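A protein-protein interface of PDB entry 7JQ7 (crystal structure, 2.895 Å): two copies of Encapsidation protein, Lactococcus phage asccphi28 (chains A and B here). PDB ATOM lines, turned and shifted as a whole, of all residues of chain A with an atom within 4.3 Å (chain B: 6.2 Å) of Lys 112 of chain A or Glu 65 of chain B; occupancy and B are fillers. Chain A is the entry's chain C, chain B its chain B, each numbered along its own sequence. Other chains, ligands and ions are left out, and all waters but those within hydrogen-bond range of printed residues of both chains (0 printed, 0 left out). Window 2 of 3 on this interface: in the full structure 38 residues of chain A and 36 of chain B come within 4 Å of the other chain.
The backbone carbonyl oxygen (O) of Glu 63 of chain B lies within hydrogen-bond range of the side-chain amide nitrogen (ND2) of Asn 135 of chain A, 3.4 Å away. The side-chain amino group (NZ) of Lys 112 of chain A is in salt-bridge range of the side-chain carboxylate (OE2) of Glu 65 of chain B. The backbone NH (N) of Glu 65 of chain B lies within hydrogen-bond range of the side-chain amide oxygen (OD1) of Asn 135 of chain A.
Of the 10 printed residues of chain A, 2 touch a printed residue of chain B.
NZ of Lys 66 of chain B sits at hydrogen-bond distance from O of Leu 64 of chain B (3.1 Å). The side-chain amino group (NZ) of Lys 112 of chain A sits close to the backbone carbonyl oxygen (O) of Arg 110 of chain A (3.5 Å).
Among the printed residues, pairs that only touch across the chains: Asn 135 of chain A with Leu 64 of chain B (2.9 Å).
Of the printed residues of chain B, Asn 135 of chain A touches Glu 63 (3.4 Å), Leu 64 (2.9 Å) and Glu 65 (3.5 Å). Printed residues of chain A within 4 Å of Glu 63 of chain B: Asn 135 (3.4 Å). Of the printed residues of chain A, Leu 64 of chain B touches Asn 135 (2.9 Å). Glu 65 of chain B touches just these residues of chain A: Lys 112 and Asn 135. The nearest printed residue of chain B that does not touch Lys 112 of chain A is Asn 68 of chain B (6.6 Å).
No position is printed for both chains. Of the 4 pairs that touch across the chains among the printed residues, none has its exchanged pair printed and touching as well.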
ATOM      1  N   LYS A 107      34.668 -17.269 -23.584  1.00  0.00           N
ATOM      2  CA  LYS A 107      33.534 -16.458 -23.176  1.00  0.00           C
ATOM      3  C   LYS A 107      32.894 -17.091 -21.951  1.00  0.00           C
ATOM      4  O   LYS A 107      32.785 -18.319 -21.863  1.00  0.00           O
ATOM      5  CB  LYS A 107      32.529 -16.349 -24.325  1.00  0.00           C
ATOM      6  CG  LYS A 107      31.303 -15.488 -24.059  1.00  0.00           C
ATOM      7  CD  LYS A 107      30.462 -15.382 -25.333  1.00  0.00           C
ATOM      8  CE  LYS A 107      29.116 -14.725 -25.080  1.00  0.00           C
ATOM      9  NZ  LYS A 107      28.228 -14.809 -26.279  1.00  0.00           N
ATOM     10  N   ALA A 108      32.487 -16.259 -21.001  1.00  0.00           N
ATOM     11  CA  ALA A 108      31.812 -16.727 -19.796  1.00  0.00           C
ATOM     12  C   ALA A 108      30.448 -16.053 -19.738  1.00  0.00           C
ATOM     13  O   ALA A 108      30.363 -14.828 -19.597  1.00  0.00           O
ATOM     14  CB  ALA A 108      32.634 -16.412 -18.547  1.00  0.00           C
ATOM     15  N   ILE A 109      29.381 -16.840 -19.863  1.00  0.00           N
ATOM     16  CA  ILE A 109      28.025 -16.318 -19.745  1.00  0.00           C
ATOM     17  C   ILE A 109      27.127 -17.383 -19.130  1.00  0.00           C
ATOM     18  O   ILE A 109      27.329 -18.583 -19.323  1.00  0.00           O
ATOM     19  CB  ILE A 109      27.496 -15.806 -21.110  1.00  0.00           C
ATOM     20  CG1 ILE A 109      27.322 -16.952 -22.100  1.00  0.00           C
ATOM     21  CG2 ILE A 109      28.412 -14.730 -21.679  1.00  0.00           C
ATOM     22  CD1 ILE A 109      25.933 -17.522 -22.117  1.00  0.00           C
ATOM     23  N   ARG A 110      26.151 -16.920 -18.350  1.00  0.00           N
ATOM     24  CA  ARG A 110      25.148 -17.756 -17.688  1.00  0.00           C
ATOM     25  C   ARG A 110      25.796 -18.920 -16.930  1.00  0.00           C
ATOM     26  O   ARG A 110      25.519 -20.100 -17.155  1.00  0.00           O
ATOM     27  CB  ARG A 110      24.083 -18.228 -18.691  1.00  0.00           C
ATOM     28  CG  ARG A 110      24.494 -19.295 -19.676  1.00  0.00           C
ATOM     29  CD  ARG A 110      23.342 -19.649 -20.647  1.00  0.00           C
ATOM     30  NE  ARG A 110      23.699 -20.827 -21.432  1.00  0.00           N
ATOM     31  CZ  ARG A 110      24.120 -20.801 -22.695  1.00  0.00           C
ATOM     32  NH1 ARG A 110      24.211 -19.652 -23.359  1.00  0.00           N
ATOM     33  NH2 ARG A 110      24.442 -21.937 -23.299  1.00  0.00           N
ATOM     34  N   ASN A 111      26.669 -18.542 -15.994  1.00  0.00           N
ATOM     35  CA  ASN A 111      27.330 -19.477 -15.078  1.00  0.00           C
ATOM     36  C   ASN A 111      27.990 -20.642 -15.814  1.00  0.00           C
ATOM     37  O   ASN A 111      28.006 -21.780 -15.335  1.00  0.00           O
ATOM     38  CB  ASN A 111      26.343 -19.993 -14.025  1.00  0.00           C
ATOM     39  CG  ASN A 111      25.843 -18.894 -13.099  1.00  0.00           C
ATOM     40  OD1 ASN A 111      25.538 -17.781 -13.538  1.00  0.00           O
ATOM     41  ND2 ASN A 111      25.766 -19.202 -11.802  1.00  0.00           N
ATOM     42  N   LYS A 112      28.551 -20.349 -16.983  1.00  0.00           N
ATOM     43  CA  LYS A 112      29.315 -21.319 -17.753  1.00  0.00           C
ATOM     44  C   LYS A 112      30.503 -20.591 -18.362  1.00  0.00           C
ATOM     45  O   LYS A 112      30.463 -19.374 -18.568  1.00  0.00           O
ATOM     46  CB  LYS A 112      28.482 -21.955 -18.865  1.00  0.00           C
ATOM     47  CG  LYS A 112      27.317 -22.782 -18.380  1.00  0.00           C
ATOM     48  CD  LYS A 112      26.526 -23.321 -19.559  1.00  0.00           C
ATOM     49  CE  LYS A 112      25.265 -24.031 -19.107  1.00  0.00           C
ATOM     50  NZ  LYS A 112      24.316 -23.081 -18.441  1.00  0.00           N
ATOM     51  N   ILE A 113      31.555 -21.340 -18.679  1.00  0.00           N
ATOM     52  CA  ILE A 113      32.702 -20.801 -19.403  1.00  0.00           C
ATOM     53  C   ILE A 113      32.893 -21.629 -20.664  1.00  0.00           C
ATOM     54  O   ILE A 113      32.853 -22.863 -20.615  1.00  0.00           O
ATOM     55  CB  ILE A 113      33.982 -20.795 -18.548  1.00  0.00           C
ATOM     56  CG1 ILE A 113      33.780 -19.928 -17.306  1.00  0.00           C
ATOM     57  CG2 ILE A 113      35.156 -20.275 -19.361  1.00  0.00           C
ATOM     58  CD1 ILE A 113      34.981 -19.871 -16.399  1.00  0.00           C
ATOM     59  N   PHE A 114      33.090 -20.950 -21.789  1.00  0.00           N
ATOM     60  CA  PHE A 114      33.209 -21.600 -23.082  1.00  0.00           C
ATOM     61  C   PHE A 114      34.582 -21.343 -23.691  1.00  0.00           C
ATOM     62  O   PHE A 114      35.181 -20.280 -23.493  1.00  0.00           O
ATOM     63  CB  PHE A 114      32.125 -21.097 -24.046  1.00  0.00           C
ATOM     64  CG  PHE A 114      30.727 -21.292 -23.546  1.00  0.00           C
ATOM     65  CD1 PHE A 114      30.148 -20.367 -22.701  1.00  0.00           C
ATOM     66  CD2 PHE A 114      29.986 -22.395 -23.934  1.00  0.00           C
ATOM     67  CE1 PHE A 114      28.854 -20.543 -22.239  1.00  0.00           C
ATOM     68  CE2 PHE A 114      28.695 -22.574 -23.478  1.00  0.00           C
ATOM     69  CZ  PHE A 114      28.129 -21.646 -22.628  1.00  0.00           C
ATOM     70  N   VAL A 121      33.626 -25.350 -18.502  1.00  0.00           N
ATOM     71  CA  VAL A 121      33.431 -25.274 -17.058  1.00  0.00           C
ATOM     72  C   VAL A 121      31.958 -25.067 -16.749  1.00  0.00           C
ATOM     73  O   VAL A 121      31.335 -24.134 -17.266  1.00  0.00           O
ATOM     74  CB  VAL A 121      34.259 -24.137 -16.430  1.00  0.00           C
ATOM     75  CG1 VAL A 121      34.041 -24.098 -14.924  1.00  0.00           C
ATOM     76  CG2 VAL A 121      35.722 -24.304 -16.775  1.00  0.00           C
ATOM     77  N   ASN A 135      19.612 -33.593 -15.437  1.00  0.00           N
ATOM     78  CA  ASN A 135      20.575 -32.810 -16.194  1.00  0.00           C
ATOM     79  C   ASN A 135      21.580 -33.739 -16.868  1.00  0.00           C
ATOM     80  O   ASN A 135      21.774 -34.889 -16.467  1.00  0.00           O
ATOM     81  CB  ASN A 135      21.290 -31.804 -15.291  1.00  0.00           C
ATOM     82  CG  ASN A 135      20.436 -30.579 -14.996  1.00  0.00           C
ATOM     83  OD1 ASN A 135      19.246 -30.550 -15.315  1.00  0.00           O
ATOM     84  ND2 ASN A 135      21.039 -29.564 -14.387  1.00  0.00           N
ATOM     85  N   ILE B  61      12.901 -26.075 -12.888  1.00  0.00           N
ATOM     86  CA  ILE B  61      13.085 -25.770 -14.304  1.00  0.00           C
ATOM     87  C   ILE B  61      14.214 -24.771 -14.521  1.00  0.00           C
ATOM     88  O   ILE B  61      15.034 -24.947 -15.425  1.00  0.00           O
ATOM     89  CB  ILE B  61      11.757 -25.265 -14.908  1.00  0.00           C
ATOM     90  CG1 ILE B  61      10.779 -26.435 -15.053  1.00  0.00           C
ATOM     91  CG2 ILE B  61      11.994 -24.612 -16.255  1.00  0.00           C
ATOM     92  CD1 ILE B  61       9.439 -26.081 -15.643  1.00  0.00           C
ATOM     93  N   ASP B  62      14.291 -23.722 -13.700  1.00  0.00           N
ATOM     94  CA  ASP B  62      15.355 -22.736 -13.866  1.00  0.00           C
ATOM     95  C   ASP B  62      16.730 -23.389 -13.759  1.00  0.00           C
ATOM     96  O   ASP B  62      17.631 -23.102 -14.556  1.00  0.00           O
ATOM     97  CB  ASP B  62      15.200 -21.613 -12.840  1.00  0.00           C
ATOM     98  CG  ASP B  62      13.891 -20.863 -12.988  1.00  0.00           C
ATOM     99  OD1 ASP B  62      13.306 -20.903 -14.094  1.00  0.00           O
ATOM    100  OD2 ASP B  62      13.464 -20.209 -12.012  1.00  0.00           O
ATOM    101  N   GLU B  63      16.916 -24.256 -12.758  1.00  0.00           N
ATOM    102  CA  GLU B  63      18.175 -24.971 -12.602  1.00  0.00           C
ATOM    103  C   GLU B  63      18.373 -26.050 -13.658  1.00  0.00           C
ATOM    104  O   GLU B  63      19.477 -26.594 -13.768  1.00  0.00           O
ATOM    105  CB  GLU B  63      18.261 -25.591 -11.209  1.00  0.00           C
ATOM    106  CG  GLU B  63      18.408 -24.564 -10.103  1.00  0.00           C
ATOM    107  CD  GLU B  63      19.613 -23.660 -10.294  1.00  0.00           C
ATOM    108  OE1 GLU B  63      20.562 -24.060 -11.005  1.00  0.00           O
ATOM    109  OE2 GLU B  63      19.600 -22.538  -9.743  1.00  0.00           O
ATOM    110  N   LEU B  64      17.339 -26.387 -14.420  1.00  0.00           N
ATOM    111  CA  LEU B  64      17.485 -27.386 -15.466  1.00  0.00           C
ATOM    112  C   LEU B  64      18.291 -26.814 -16.626  1.00  0.00           C
ATOM    113  O   LEU B  64      18.074 -25.680 -17.059  1.00  0.00           O
ATOM    114  CB  LEU B  64      16.114 -27.842 -15.945  1.00  0.00           C
ATOM    115  CG  LEU B  64      16.123 -28.757 -17.166  1.00  0.00           C
ATOM    116  CD1 LEU B  64      16.912 -30.022 -16.903  1.00  0.00           C
ATOM    117  CD2 LEU B  64      14.682 -29.064 -17.557  1.00  0.00           C
ATOM    118  N   GLU B  65      19.217 -27.613 -17.140  1.00  0.00           N
ATOM    119  CA  GLU B  65      20.004 -27.217 -18.301  1.00  0.00           C
ATOM    120  C   GLU B  65      19.194 -27.552 -19.545  1.00  0.00           C
ATOM    121  O   GLU B  65      18.997 -28.729 -19.864  1.00  0.00           O
ATOM    122  CB  GLU B  65      21.347 -27.936 -18.301  1.00  0.00           C
ATOM    123  CG  GLU B  65      22.352 -27.399 -17.285  1.00  0.00           C
ATOM    124  CD  GLU B  65      22.983 -26.083 -17.704  1.00  0.00           C
ATOM    125  OE1 GLU B  65      23.137 -25.855 -18.923  1.00  0.00           O
ATOM    126  OE2 GLU B  65      23.338 -25.282 -16.814  1.00  0.00           O
ATOM    127  N   LYS B  66      18.734 -26.522 -20.256  1.00  0.00           N
ATOM    128  CA  LYS B  66      17.823 -26.743 -21.372  1.00  0.00           C
ATOM    129  C   LYS B  66      18.556 -27.262 -22.602  1.00  0.00           C
ATOM    130  O   LYS B  66      18.135 -28.254 -23.208  1.00  0.00           O
ATOM    131  CB  LYS B  66      17.082 -25.449 -21.723  1.00  0.00           C
ATOM    132  CG  LYS B  66      16.660 -24.584 -20.544  1.00  0.00           C
ATOM    133  CD  LYS B  66      15.716 -25.292 -19.596  1.00  0.00           C
ATOM    134  CE  LYS B  66      15.080 -24.293 -18.628  1.00  0.00           C
ATOM    135  NZ  LYS B  66      16.084 -23.451 -17.902  1.00  0.00           N
ATOM    136  N   ASN B  67      19.649 -26.599 -22.995  1.00  0.00           N
ATOM    137  CA  ASN B  67      20.327 -26.975 -24.230  1.00  0.00           C
ATOM    138  C   ASN B  67      20.695 -28.452 -24.245  1.00  0.00           C
ATOM    139  O   ASN B  67      20.800 -29.061 -25.317  1.00  0.00           O
ATOM    140  CB  ASN B  67      21.590 -26.135 -24.429  1.00  0.00           C
ATOM    141  CG  ASN B  67      22.182 -26.303 -25.821  1.00  0.00           C
ATOM    142  OD1 ASN B  67      21.458 -26.524 -26.799  1.00  0.00           O
ATOM    143  ND2 ASN B  67      23.505 -26.199 -25.918  1.00  0.00           N
ATOM    144  N   ASN B  68      20.900 -29.035 -23.073  1.00  0.00           N
ATOM    145  CA  ASN B  68      21.308 -30.421 -22.932  1.00  0.00           C
ATOM    146  C   ASN B  68      20.117 -31.367 -22.837  1.00  0.00           C
ATOM    147  O   ASN B  68      20.315 -32.582 -22.736  1.00  0.00           O
ATOM    148  CB  ASN B  68      22.207 -30.526 -21.698  1.00  0.00           C
ATOM    149  CG  ASN B  68      23.656 -30.172 -22.005  1.00  0.00           C
ATOM    150  OD1 ASN B  68      23.969 -29.698 -23.094  1.00  0.00           O
ATOM    151  ND2 ASN B  68      24.521 -30.302 -21.009  1.00  0.00           N
ATOM    152  N   PHE B  69      18.890 -30.836 -22.891  1.00  0.00           N
ATOM    153  CA  PHE B  69      17.691 -31.672 -22.850  1.00  0.00           C
ATOM    154  C   PHE B  69      17.658 -32.625 -24.035  1.00  0.00           C
ATOM    155  O   PHE B  69      17.378 -33.819 -23.880  1.00  0.00           O
ATOM    156  CB  PHE B  69      16.445 -30.779 -22.830  1.00  0.00           C
ATOM    157  CG  PHE B  69      15.170 -31.508 -22.514  1.00  0.00           C
ATOM    158  CD1 PHE B  69      14.892 -31.920 -21.227  1.00  0.00           C
ATOM    159  CD2 PHE B  69      14.237 -31.751 -23.502  1.00  0.00           C
ATOM    160  CE1 PHE B  69      13.720 -32.582 -20.941  1.00  0.00           C
ATOM    161  CE2 PHE B  69      13.063 -32.407 -23.220  1.00  0.00           C
ATOM    162  CZ  PHE B  69      12.804 -32.824 -21.940  1.00  0.00           C
ATOM    163  N   PHE B 123       9.010 -25.794 -21.504  1.00  0.00           N
ATOM    164  CA  PHE B 123       9.358 -26.084 -20.118  1.00  0.00           C
ATOM    165  C   PHE B 123       8.522 -25.161 -19.245  1.00  0.00           C
ATOM    166  O   PHE B 123       8.762 -23.950 -19.223  1.00  0.00           O
ATOM    167  CB  PHE B 123      10.846 -25.873 -19.858  1.00  0.00           C
ATOM    168  CG  PHE B 123      11.732 -26.826 -20.600  1.00  0.00           C
ATOM    169  CD1 PHE B 123      11.929 -28.109 -20.136  1.00  0.00           C
ATOM    170  CD2 PHE B 123      12.380 -26.432 -21.746  1.00  0.00           C
ATOM    171  CE1 PHE B 123      12.745 -28.982 -20.815  1.00  0.00           C
ATOM    172  CE2 PHE B 123      13.198 -27.296 -22.424  1.00  0.00           C
ATOM    173  CZ  PHE B 123      13.384 -28.572 -21.962  1.00  0.00           C
